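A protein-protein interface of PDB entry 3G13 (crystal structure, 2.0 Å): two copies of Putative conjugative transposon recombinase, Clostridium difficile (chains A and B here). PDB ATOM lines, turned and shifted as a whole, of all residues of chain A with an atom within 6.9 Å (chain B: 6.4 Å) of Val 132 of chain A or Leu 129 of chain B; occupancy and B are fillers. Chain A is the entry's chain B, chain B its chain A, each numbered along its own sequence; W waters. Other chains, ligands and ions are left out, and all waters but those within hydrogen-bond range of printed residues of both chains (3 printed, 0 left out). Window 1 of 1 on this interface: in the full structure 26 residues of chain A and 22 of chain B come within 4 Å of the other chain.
Among the printed residues, pairs that only touch across the chains: Val 128 of chain A with Leu 125 of chain B (3.5 Å), Leu 129 of chain A with Val 132 of chain B (3.6 Å), Ser 131 of chain A with Ile 84 of chain B (3.7 Å), Thr 91 of chain A with Val 132 of chain B (3.7 Å), Val 132 of chain A with Thr 91 of chain B (3.7 Å), Val 128 of chain A with Leu 129 of chain B (3.7 Å), Val 128 of chain A with Val 128 of chain B (3.8 Å), Val 132 of chain A with Leu 129 of chain B (3.8 Å), Glu 136 of chain A with Glu 136 of chain B (3.9 Å) and Val 132 of chain A with Glu 136 of chain B (3.96 Å).
Of the 14 printed residues of chain A, 7 touch a printed residue of chain B.
Hydrophobic or aromatic side chains of chain A within 4 Å of the printed part of chain B: Val 128, Leu 129 and Val 132.
Hydrophobic or aromatic side chains of chain B within 4 Å of the printed part of chain A: Ile 84, Leu 125, Val 128, Leu 129 and Val 132.
Along chain B the printed residues that touch a printed residue of chain A span positions 84 to 136.
Among the printed residues, 13 pairs touch across the chains.
OE2 of Glu 136 of chain B lies within hydrogen-bond range of OG1 of Thr 91 of chain B, 3.1 Å away.
The backbone carbonyl oxygen (O) of Val 127 of chain A is in hydrogen-bond range of the side-chain hydroxyl (OG) of Ser 131 of chain A (3.0 Å).
Of the printed residues of chain B, Thr 91 of chain A touches Val 132 (3.7 Å).
Printed residues of chain B within 4 Å of Val 128 of chain A: Leu 125 (3.5 Å), Val 128 (3.8 Å) and Leu 129 (3.7 Å).
Ser 130 of chain A touches none of the printed residues of chain B.
Of the printed residues of chain B, Ser 131 of chain A touches Ile 84.
Of chain B, only Thr 91, Leu 129 and Glu 136 come within 4 Å of Val 132 of chain A.
Gln 134 of chain A touches none of the printed residues of chain B.
Of chain A, only Val 128 (3.7 Å) and Val 132 (3.8 Å) come within 4 Å of Leu 129 of chain B.
Of the printed residues of chain A, Val 132 of chain B touches Thr 91 (3.7 Å) and Leu 129 (3.6 Å).
Printed residues of chain A within 4 Å of Glu 136 of chain B: Val 132 (3.96 Å) and Glu 136 (3.9 Å).
The side-chain amide nitrogen of Gln 135 of chain A lies within hydrogen-bond range of the backbone carbonyl oxygen of Ile 84 of chain B, 3.1 Å away.
The side-chain amide oxygen of Gln 135 of chain A sits at hydrogen-bond distance from the backbone NH of Thr 91 of chain B (3.2 Å).
The side-chain hydroxyl of Thr 94 of chain B lies within hydrogen-bond range of the side-chain amide nitrogen of Gln 135 of chain A (2.9 Å).
Water W2 lies within hydrogen-bond range of the side-chain carboxylate of Glu 136 of chain A, the side-chain hydroxyl of Thr 91 of chain A and the side-chain carboxylate of Glu 136 of chain B.
Water W3 lies within hydrogen-bond range of the side-chain amide oxygen of Gln 134 of chain A (2.7 Å), the backbone NH of Ile 84 of chain B (3.4 Å) and the side-chain hydroxyl of Ser 131 of chain A (3.5 Å).
Water W1 lies within hydrogen-bond range of O of Val 132 of chain B (3.3 Å) and OG1 of Thr 91 of chain A (3.3 Å).
Val 128 of chain A touches its own counterpart, Val 128 of chain B.
Val 128 of chain A touches Leu 129 of chain B, but with the chains exchanged Leu 129 of chain A does not touch Val 128 of chain B (4.1 Å).
Val 132 of chain A touches Glu 136 of chain B, but with the chains exchanged Glu 136 of chain A does not touch Val 132 of chain B (6.1 Å).
Glu 136 of chain A touches its own counterpart, Glu 136 of chain B.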
ATOM      1  N   ILE A  84      -8.117  16.089   1.981  1.00  0.00           N
ATOM      2  CA  ILE A  84      -7.855  14.772   1.392  1.00  0.00           C
ATOM      3  C   ILE A  84      -6.338  14.426   1.366  1.00  0.00           C
ATOM      4  O   ILE A  84      -5.933  13.288   1.654  1.00  0.00           O
ATOM      5  CB  ILE A  84      -8.477  14.710  -0.049  1.00  0.00           C
ATOM      6  CG1 ILE A  84     -10.014  14.875   0.040  1.00  0.00           C
ATOM      7  CG2 ILE A  84      -8.107  13.408  -0.743  1.00  0.00           C
ATOM      8  CD1 ILE A  84     -10.740  15.194  -1.303  1.00  0.00           C
ATOM      9  N   THR A  91      -4.971   7.363  -2.732  1.00  0.00           N
ATOM     10  CA  THR A  91      -6.341   7.248  -3.211  1.00  0.00           C
ATOM     11  C   THR A  91      -7.020   5.999  -2.711  1.00  0.00           C
ATOM     12  O   THR A  91      -8.154   6.059  -2.235  1.00  0.00           O
ATOM     13  CB  THR A  91      -6.394   7.316  -4.740  1.00  0.00           C
ATOM     14  OG1 THR A  91      -5.947   8.595  -5.110  1.00  0.00           O
ATOM     15  CG2 THR A  91      -7.836   7.118  -5.270  1.00  0.00           C
ATOM     16  N   LEU A  95     -10.360   5.996  -0.152  1.00  0.00           N
ATOM     17  CA  LEU A  95     -11.544   5.193  -0.408  1.00  0.00           C
ATOM     18  C   LEU A  95     -11.832   4.191   0.703  1.00  0.00           C
ATOM     19  O   LEU A  95     -12.955   4.120   1.194  1.00  0.00           O
ATOM     20  CB  LEU A  95     -11.432   4.467  -1.757  1.00  0.00           C
ATOM     21  CG  LEU A  95     -11.749   5.234  -3.031  1.00  0.00           C
ATOM     22  CD1 LEU A  95     -11.170   4.511  -4.268  1.00  0.00           C
ATOM     23  CD2 LEU A  95     -13.273   5.438  -3.178  1.00  0.00           C
ATOM     24  N   VAL A 127     -17.215   8.466  -6.067  1.00  0.00           N
ATOM     25  CA  VAL A 127     -17.099   8.172  -7.522  1.00  0.00           C
ATOM     26  C   VAL A 127     -15.843   8.719  -8.195  1.00  0.00           C
ATOM     27  O   VAL A 127     -15.261   8.042  -8.987  1.00  0.00           O
ATOM     28  CB  VAL A 127     -18.421   8.367  -8.436  1.00  0.00           C
ATOM     29  CG1 VAL A 127     -19.659   8.757  -7.692  1.00  0.00           C
ATOM     30  CG2 VAL A 127     -18.145   9.174  -9.744  1.00  0.00           C
ATOM     31  N   VAL A 128     -15.419   9.933  -7.883  1.00  0.00           N
ATOM     32  CA  VAL A 128     -14.222  10.522  -8.506  1.00  0.00           C
ATOM     33  C   VAL A 128     -12.965   9.732  -8.063  1.00  0.00           C
ATOM     34  O   VAL A 128     -12.100   9.407  -8.887  1.00  0.00           O
ATOM     35  CB  VAL A 128     -14.090  12.029  -8.165  1.00  0.00           C
ATOM     36  CG1 VAL A 128     -12.743  12.557  -8.578  1.00  0.00           C
ATOM     37  CG2 VAL A 128     -15.236  12.824  -8.844  1.00  0.00           C
ATOM     38  N   LEU A 129     -12.874   9.423  -6.769  1.00  0.00           N
ATOM     39  CA  LEU A 129     -11.744   8.626  -6.294  1.00  0.00           C
ATOM     40  C   LEU A 129     -11.718   7.220  -6.923  1.00  0.00           C
ATOM     41  O   LEU A 129     -10.641   6.746  -7.294  1.00  0.00           O
ATOM     42  CB  LEU A 129     -11.723   8.523  -4.771  1.00  0.00           C
ATOM     43  CG  LEU A 129     -11.498   9.769  -3.901  1.00  0.00           C
ATOM     44  CD1 LEU A 129     -11.478   9.330  -2.453  1.00  0.00           C
ATOM     45  CD2 LEU A 129     -10.255  10.555  -4.195  1.00  0.00           C
ATOM     46  N   SER A 130     -12.886   6.573  -7.018  1.00  0.00           N
ATOM     47  CA  SER A 130     -13.019   5.276  -7.709  1.00  0.00           C
ATOM     48  C   SER A 130     -12.521   5.360  -9.158  1.00  0.00           C
ATOM     49  O   SER A 130     -11.821   4.472  -9.625  1.00  0.00           O
ATOM     50  CB  SER A 130     -14.464   4.747  -7.686  1.00  0.00           C
ATOM     51  OG  SER A 130     -14.885   4.490  -6.375  1.00  0.00           O
ATOM     52  N   SER A 131     -12.858   6.445  -9.848  1.00  0.00           N
ATOM     53  CA  SER A 131     -12.366   6.720 -11.217  1.00  0.00           C
ATOM     54  C   SER A 131     -10.833   6.925 -11.292  1.00  0.00           C
ATOM     55  O   SER A 131     -10.158   6.405 -12.182  1.00  0.00           O
ATOM     56  CB  SER A 131     -13.082   7.926 -11.799  1.00  0.00           C
ATOM     57  OG  SER A 131     -14.457   7.634 -11.879  1.00  0.00           O
ATOM     58  N   VAL A 132     -10.292   7.673 -10.341  1.00  0.00           N
ATOM     59  CA  VAL A 132      -8.847   7.824 -10.255  1.00  0.00           C
ATOM     60  C   VAL A 132      -8.179   6.457 -10.068  1.00  0.00           C
ATOM     61  O   VAL A 132      -7.209   6.155 -10.767  1.00  0.00           O
ATOM     62  CB  VAL A 132      -8.392   8.797  -9.124  1.00  0.00           C
ATOM     63  CG1 VAL A 132      -6.892   8.623  -8.839  1.00  0.00           C
ATOM     64  CG2 VAL A 132      -8.693  10.229  -9.507  1.00  0.00           C
ATOM     65  N   ALA A 133      -8.704   5.633  -9.159  1.00  0.00           N
ATOM     66  CA  ALA A 133      -8.136   4.308  -8.966  1.00  0.00           C
ATOM     67  C   ALA A 133      -8.248   3.468 -10.258  1.00  0.00           C
ATOM     68  O   ALA A 133      -7.261   2.845 -10.657  1.00  0.00           O
ATOM     69  CB  ALA A 133      -8.772   3.591  -7.789  1.00  0.00           C
ATOM     70  N   GLN A 134      -9.426   3.478 -10.899  1.00  0.00           N
ATOM     71  CA  GLN A 134      -9.680   2.725 -12.148  1.00  0.00           C
ATOM     72  C   GLN A 134      -8.731   3.204 -13.263  1.00  0.00           C
ATOM     73  O   GLN A 134      -8.178   2.395 -13.995  1.00  0.00           O
ATOM     74  CB  GLN A 134     -11.174   2.839 -12.582  1.00  0.00           C
ATOM     75  CG  GLN A 134     -11.532   2.207 -13.954  1.00  0.00           C
ATOM     76  CD  GLN A 134     -12.907   2.637 -14.577  1.00  0.00           C
ATOM     77  OE1 GLN A 134     -13.519   3.662 -14.211  1.00  0.00           O
ATOM     78  NE2 GLN A 134     -13.373   1.835 -15.546  1.00  0.00           N
ATOM     79  N   GLN A 135      -8.575   4.521 -13.390  1.00  0.00           N
ATOM     80  CA  GLN A 135      -7.620   5.162 -14.293  1.00  0.00           C
ATOM     81  C   GLN A 135      -6.178   4.666 -14.144  1.00  0.00           C
ATOM     82  O   GLN A 135      -5.464   4.507 -15.166  1.00  0.00           O
ATOM     83  CB  GLN A 135      -7.675   6.686 -14.124  1.00  0.00           C
ATOM     84  CG  GLN A 135      -6.796   7.492 -15.043  1.00  0.00           C
ATOM     85  CD  GLN A 135      -6.982   8.983 -14.810  1.00  0.00           C
ATOM     86  OE1 GLN A 135      -6.507   9.521 -13.820  1.00  0.00           O
ATOM     87  NE2 GLN A 135      -7.701   9.644 -15.699  1.00  0.00           N
ATOM     88  N   GLU A 136      -5.757   4.405 -12.899  1.00  0.00           N
ATOM     89  CA  GLU A 136      -4.416   3.844 -12.682  1.00  0.00           C
ATOM     90  C   GLU A 136      -4.348   2.423 -13.237  1.00  0.00           C
ATOM     91  O   GLU A 136      -3.433   2.080 -14.000  1.00  0.00           O
ATOM     92  CB  GLU A 136      -3.978   3.890 -11.202  1.00  0.00           C
ATOM     93  CG  GLU A 136      -3.904   5.310 -10.634  1.00  0.00           C
ATOM     94  CD  GLU A 136      -3.527   5.371  -9.135  1.00  0.00           C
ATOM     95  OE1 GLU A 136      -2.774   4.476  -8.678  1.00  0.00           O
ATOM     96  OE2 GLU A 136      -3.988   6.308  -8.426  1.00  0.00           O
ATOM     97  N   VAL A 137      -5.354   1.625 -12.903  1.00  0.00           N
ATOM     98  CA  VAL A 137      -5.410   0.240 -13.324  1.00  0.00           C
ATOM     99  C   VAL A 137      -5.361   0.113 -14.855  1.00  0.00           C
ATOM    100  O   VAL A 137      -4.635  -0.752 -15.396  1.00  0.00           O
ATOM    101  CB  VAL A 137      -6.639  -0.476 -12.673  1.00  0.00           C
ATOM    102  CG1 VAL A 137      -6.916  -1.811 -13.310  1.00  0.00           C
ATOM    103  CG2 VAL A 137      -6.415  -0.639 -11.176  1.00  0.00           C
ATOM    104  N   ILE B  84     -13.640   8.796 -16.810  1.00  0.00           N
ATOM    105  CA  ILE B  84     -12.398   9.509 -16.559  1.00  0.00           C
ATOM    106  C   ILE B  84     -11.148   8.697 -16.999  1.00  0.00           C
ATOM    107  O   ILE B  84     -10.186   9.264 -17.532  1.00  0.00           O
ATOM    108  CB  ILE B  84     -12.287   9.918 -15.033  1.00  0.00           C
ATOM    109  CG1 ILE B  84     -13.233  11.104 -14.750  1.00  0.00           C
ATOM    110  CG2 ILE B  84     -10.857  10.304 -14.687  1.00  0.00           C
ATOM    111  CD1 ILE B  84     -13.666  11.296 -13.273  1.00  0.00           C
ATOM    112  N   THR B  91      -4.142  11.649 -13.203  1.00  0.00           N
ATOM    113  CA  THR B  91      -4.815  12.778 -12.571  1.00  0.00           C
ATOM    114  C   THR B  91      -4.378  14.136 -13.127  1.00  0.00           C
ATOM    115  O   THR B  91      -5.223  14.978 -13.440  1.00  0.00           O
ATOM    116  CB  THR B  91      -4.649  12.714 -11.040  1.00  0.00           C
ATOM    117  OG1 THR B  91      -5.263  11.505 -10.585  1.00  0.00           O
ATOM    118  CG2 THR B  91      -5.355  13.893 -10.369  1.00  0.00           C
ATOM    119  N   LEU B  92      -3.060  14.334 -13.255  1.00  0.00           N
ATOM    120  CA  LEU B  92      -2.514  15.579 -13.765  1.00  0.00           C
ATOM    121  C   LEU B  92      -2.995  15.938 -15.189  1.00  0.00           C
ATOM    122  O   LEU B  92      -3.296  17.100 -15.474  1.00  0.00           O
ATOM    123  CB  LEU B  92      -0.981  15.566 -13.694  1.00  0.00           C
ATOM    124  CG  LEU B  92      -0.434  15.859 -12.293  1.00  0.00           C
ATOM    125  CD1 LEU B  92       1.083  15.697 -12.297  1.00  0.00           C
ATOM    126  CD2 LEU B  92      -0.803  17.281 -11.877  1.00  0.00           C
ATOM    127  N   THR B  94      -5.789  14.700 -16.565  1.00  0.00           N
ATOM    128  CA  THR B  94      -7.251  14.909 -16.447  1.00  0.00           C
ATOM    129  C   THR B  94      -7.535  16.375 -16.102  1.00  0.00           C
ATOM    130  O   THR B  94      -8.387  17.021 -16.726  1.00  0.00           O
ATOM    131  CB  THR B  94      -7.925  13.973 -15.383  1.00  0.00           C
ATOM    132  OG1 THR B  94      -7.594  12.590 -15.625  1.00  0.00           O
ATOM    133  CG2 THR B  94      -9.434  14.131 -15.421  1.00  0.00           C
ATOM    134  N   LEU B  95      -6.811  16.886 -15.104  1.00  0.00           N
ATOM    135  CA  LEU B  95      -6.861  18.295 -14.710  1.00  0.00           C
ATOM    136  C   LEU B  95      -6.566  19.236 -15.842  1.00  0.00           C
ATOM    137  O   LEU B  95      -7.337  20.157 -16.121  1.00  0.00           O
ATOM    138  CB  LEU B  95      -5.844  18.571 -13.571  1.00  0.00           C
ATOM    139  CG  LEU B  95      -6.291  18.149 -12.179  1.00  0.00           C
ATOM    140  CD1 LEU B  95      -5.096  18.247 -11.170  1.00  0.00           C
ATOM    141  CD2 LEU B  95      -7.470  19.062 -11.784  1.00  0.00           C
ATOM    142  N   VAL B  98      -9.269  18.932 -18.745  1.00  0.00           N
ATOM    143  CA  VAL B  98     -10.591  19.417 -18.326  1.00  0.00           C
ATOM    144  C   VAL B  98     -10.559  20.964 -18.171  1.00  0.00           C
ATOM    145  O   VAL B  98     -11.423  21.660 -18.693  1.00  0.00           O
ATOM    146  CB  VAL B  98     -11.105  18.741 -17.067  1.00  0.00           C
ATOM    147  CG1 VAL B  98     -12.352  19.514 -16.515  1.00  0.00           C
ATOM    148  CG2 VAL B  98     -11.431  17.254 -17.362  1.00  0.00           C
ATOM    149  N   LEU B 124     -16.445  20.671  -8.158  1.00  0.00           N
ATOM    150  CA  LEU B 124     -16.009  19.762  -7.098  1.00  0.00           C
ATOM    151  C   LEU B 124     -15.070  18.659  -7.648  1.00  0.00           C
ATOM    152  O   LEU B 124     -14.161  18.254  -6.965  1.00  0.00           O
ATOM    153  CB  LEU B 124     -17.193  19.160  -6.359  1.00  0.00           C
ATOM    154  CG  LEU B 124     -16.920  18.570  -4.961  1.00  0.00           C
ATOM    155  CD1 LEU B 124     -16.328  19.667  -4.002  1.00  0.00           C
ATOM    156  CD2 LEU B 124     -18.199  17.925  -4.410  1.00  0.00           C
ATOM    157  N   LEU B 125     -15.330  18.160  -8.860  1.00  0.00           N
ATOM    158  CA  LEU B 125     -14.438  17.189  -9.508  1.00  0.00           C
ATOM    159  C   LEU B 125     -13.024  17.738  -9.529  1.00  0.00           C
ATOM    160  O   LEU B 125     -12.083  17.065  -9.082  1.00  0.00           O
ATOM    161  CB  LEU B 125     -14.939  16.834 -10.924  1.00  0.00           C
ATOM    162  CG  LEU B 125     -13.949  16.124 -11.858  1.00  0.00           C
ATOM    163  CD1 LEU B 125     -13.790  14.708 -11.375  1.00  0.00           C
ATOM    164  CD2 LEU B 125     -14.509  16.142 -13.305  1.00  0.00           C
ATOM    165  N   LEU B 126     -12.891  18.989  -9.975  1.00  0.00           N
ATOM    166  CA  LEU B 126     -11.593  19.632 -10.135  1.00  0.00           C
ATOM    167  C   LEU B 126     -10.891  19.907  -8.800  1.00  0.00           C
ATOM    168  O   LEU B 126      -9.656  19.765  -8.701  1.00  0.00           O
ATOM    169  CB  LEU B 126     -11.753  20.914 -10.947  1.00  0.00           C
ATOM    170  CG  LEU B 126     -12.119  20.712 -12.428  1.00  0.00           C
ATOM    171  CD1 LEU B 126     -12.331  22.090 -13.025  1.00  0.00           C
ATOM    172  CD2 LEU B 126     -11.012  19.919 -13.204  1.00  0.00           C
ATOM    173  N   VAL B 127     -11.679  20.263  -7.781  1.00  0.00           N
ATOM    174  CA  VAL B 127     -11.162  20.430  -6.419  1.00  0.00           C
ATOM    175  C   VAL B 127     -10.575  19.107  -5.915  1.00  0.00           C
ATOM    176  O   VAL B 127      -9.457  19.082  -5.379  1.00  0.00           O
ATOM    177  CB  VAL B 127     -12.270  20.986  -5.423  1.00  0.00           C
ATOM    178  CG1 VAL B 127     -11.888  20.703  -3.978  1.00  0.00           C
ATOM    179  CG2 VAL B 127     -12.456  22.489  -5.582  1.00  0.00           C
ATOM    180  N   VAL B 128     -11.328  18.013  -6.083  1.00  0.00           N
ATOM    181  CA  VAL B 128     -10.928  16.679  -5.616  1.00  0.00           C
ATOM    182  C   VAL B 128      -9.695  16.188  -6.379  1.00  0.00           C
ATOM    183  O   VAL B 128      -8.748  15.710  -5.778  1.00  0.00           O
ATOM    184  CB  VAL B 128     -12.073  15.603  -5.705  1.00  0.00           C
ATOM    185  CG1 VAL B 128     -11.537  14.207  -5.396  1.00  0.00           C
ATOM    186  CG2 VAL B 128     -13.197  15.908  -4.720  1.00  0.00           C
ATOM    187  N   LEU B 129      -9.713  16.331  -7.702  1.00  0.00           N
ATOM    188  CA  LEU B 129      -8.541  15.993  -8.527  1.00  0.00           C
ATOM    189  C   LEU B 129      -7.289  16.803  -8.167  1.00  0.00           C
ATOM    190  O   LEU B 129      -6.208  16.255  -8.225  1.00  0.00           O
ATOM    191  CB  LEU B 129      -8.805  16.149 -10.018  1.00  0.00           C
ATOM    192  CG  LEU B 129      -9.902  15.280 -10.639  1.00  0.00           C
ATOM    193  CD1 LEU B 129      -9.984  15.510 -12.151  1.00  0.00           C
ATOM    194  CD2 LEU B 129      -9.673  13.834 -10.297  1.00  0.00           C
ATOM    195  N   SER B 130      -7.447  18.092  -7.836  1.00  0.00           N
ATOM    196  CA  SER B 130      -6.313  18.915  -7.432  1.00  0.00           C
ATOM    197  C   SER B 130      -5.678  18.388  -6.135  1.00  0.00           C
ATOM    198  O   SER B 130      -4.451  18.376  -6.020  1.00  0.00           O
ATOM    199  CB  SER B 130      -6.694  20.382  -7.237  1.00  0.00           C
ATOM    200  OG  SER B 130      -7.311  20.918  -8.394  1.00  0.00           O
ATOM    201  N   SER B 131      -6.513  17.954  -5.178  1.00  0.00           N
ATOM    202  CA  SER B 131      -6.031  17.425  -3.895  1.00  0.00           C
ATOM    203  C   SER B 131      -5.374  16.072  -4.092  1.00  0.00           C
ATOM    204  O   SER B 131      -4.330  15.803  -3.526  1.00  0.00           O
ATOM    205  CB  SER B 131      -7.157  17.322  -2.856  1.00  0.00           C
ATOM    206  OG  SER B 131      -7.348  18.605  -2.280  1.00  0.00           O
ATOM    207  N   VAL B 132      -6.002  15.238  -4.916  1.00  0.00           N
ATOM    208  CA  VAL B 132      -5.441  13.949  -5.305  1.00  0.00           C
ATOM    209  C   VAL B 132      -4.073  14.114  -5.987  1.00  0.00           C
ATOM    210  O   VAL B 132      -3.125  13.445  -5.608  1.00  0.00           O
ATOM    211  CB  VAL B 132      -6.419  13.160  -6.191  1.00  0.00           C
ATOM    212  CG1 VAL B 132      -5.757  11.941  -6.763  1.00  0.00           C
ATOM    213  CG2 VAL B 132      -7.662  12.724  -5.373  1.00  0.00           C
ATOM    214  N   ALA B 133      -3.978  15.003  -6.974  1.00  0.00           N
ATOM    215  CA  ALA B 133      -2.724  15.254  -7.706  1.00  0.00           C
ATOM    216  C   ALA B 133      -1.583  15.804  -6.818  1.00  0.00           C
ATOM    217  O   ALA B 133      -0.426  15.446  -7.018  1.00  0.00           O
ATOM    218  CB  ALA B 133      -2.957  16.175  -8.887  1.00  0.00           C
ATOM    219  N   GLN B 134      -1.911  16.672  -5.857  1.00  0.00           N
ATOM    220  CA  GLN B 134      -0.904  17.197  -4.927  1.00  0.00           C
ATOM    221  C   GLN B 134      -0.305  16.064  -4.096  1.00  0.00           C
ATOM    222  O   GLN B 134       0.904  15.984  -3.917  1.00  0.00           O
ATOM    223  CB  GLN B 134      -1.494  18.271  -4.004  1.00  0.00           C
ATOM    224  CG  GLN B 134      -0.479  18.909  -3.012  1.00  0.00           C
ATOM    225  CD  GLN B 134       0.688  19.622  -3.708  1.00  0.00           C
ATOM    226  OE1 GLN B 134       0.543  20.142  -4.817  1.00  0.00           O
ATOM    227  NE2 GLN B 134       1.849  19.659  -3.047  1.00  0.00           N
ATOM    228  N   GLU B 136      -0.329  12.787  -4.910  1.00  0.00           N
ATOM    229  CA  GLU B 136       0.404  11.895  -5.798  1.00  0.00           C
ATOM    230  C   GLU B 136       1.805  12.461  -6.079  1.00  0.00           C
ATOM    231  O   GLU B 136       2.763  11.721  -6.079  1.00  0.00           O
ATOM    232  CB  GLU B 136      -0.309  11.704  -7.135  1.00  0.00           C
ATOM    233  CG  GLU B 136      -1.616  10.912  -7.095  1.00  0.00           C
ATOM    234  CD  GLU B 136      -2.315  10.933  -8.464  1.00  0.00           C
ATOM    235  OE1 GLU B 136      -1.927  11.749  -9.321  1.00  0.00           O
ATOM    236  OE2 GLU B 136      -3.249  10.157  -8.684  1.00  0.00           O
HETATM  237  O   HOH W   1      -3.551  10.634  -3.978  1.00  0.00           O
HETATM  238  O   HOH W   2      -4.058   8.320  -6.924  1.00  0.00           O
HETATM  239  O   HOH W   3     -12.914   6.222 -14.632  1.00  0.00           O
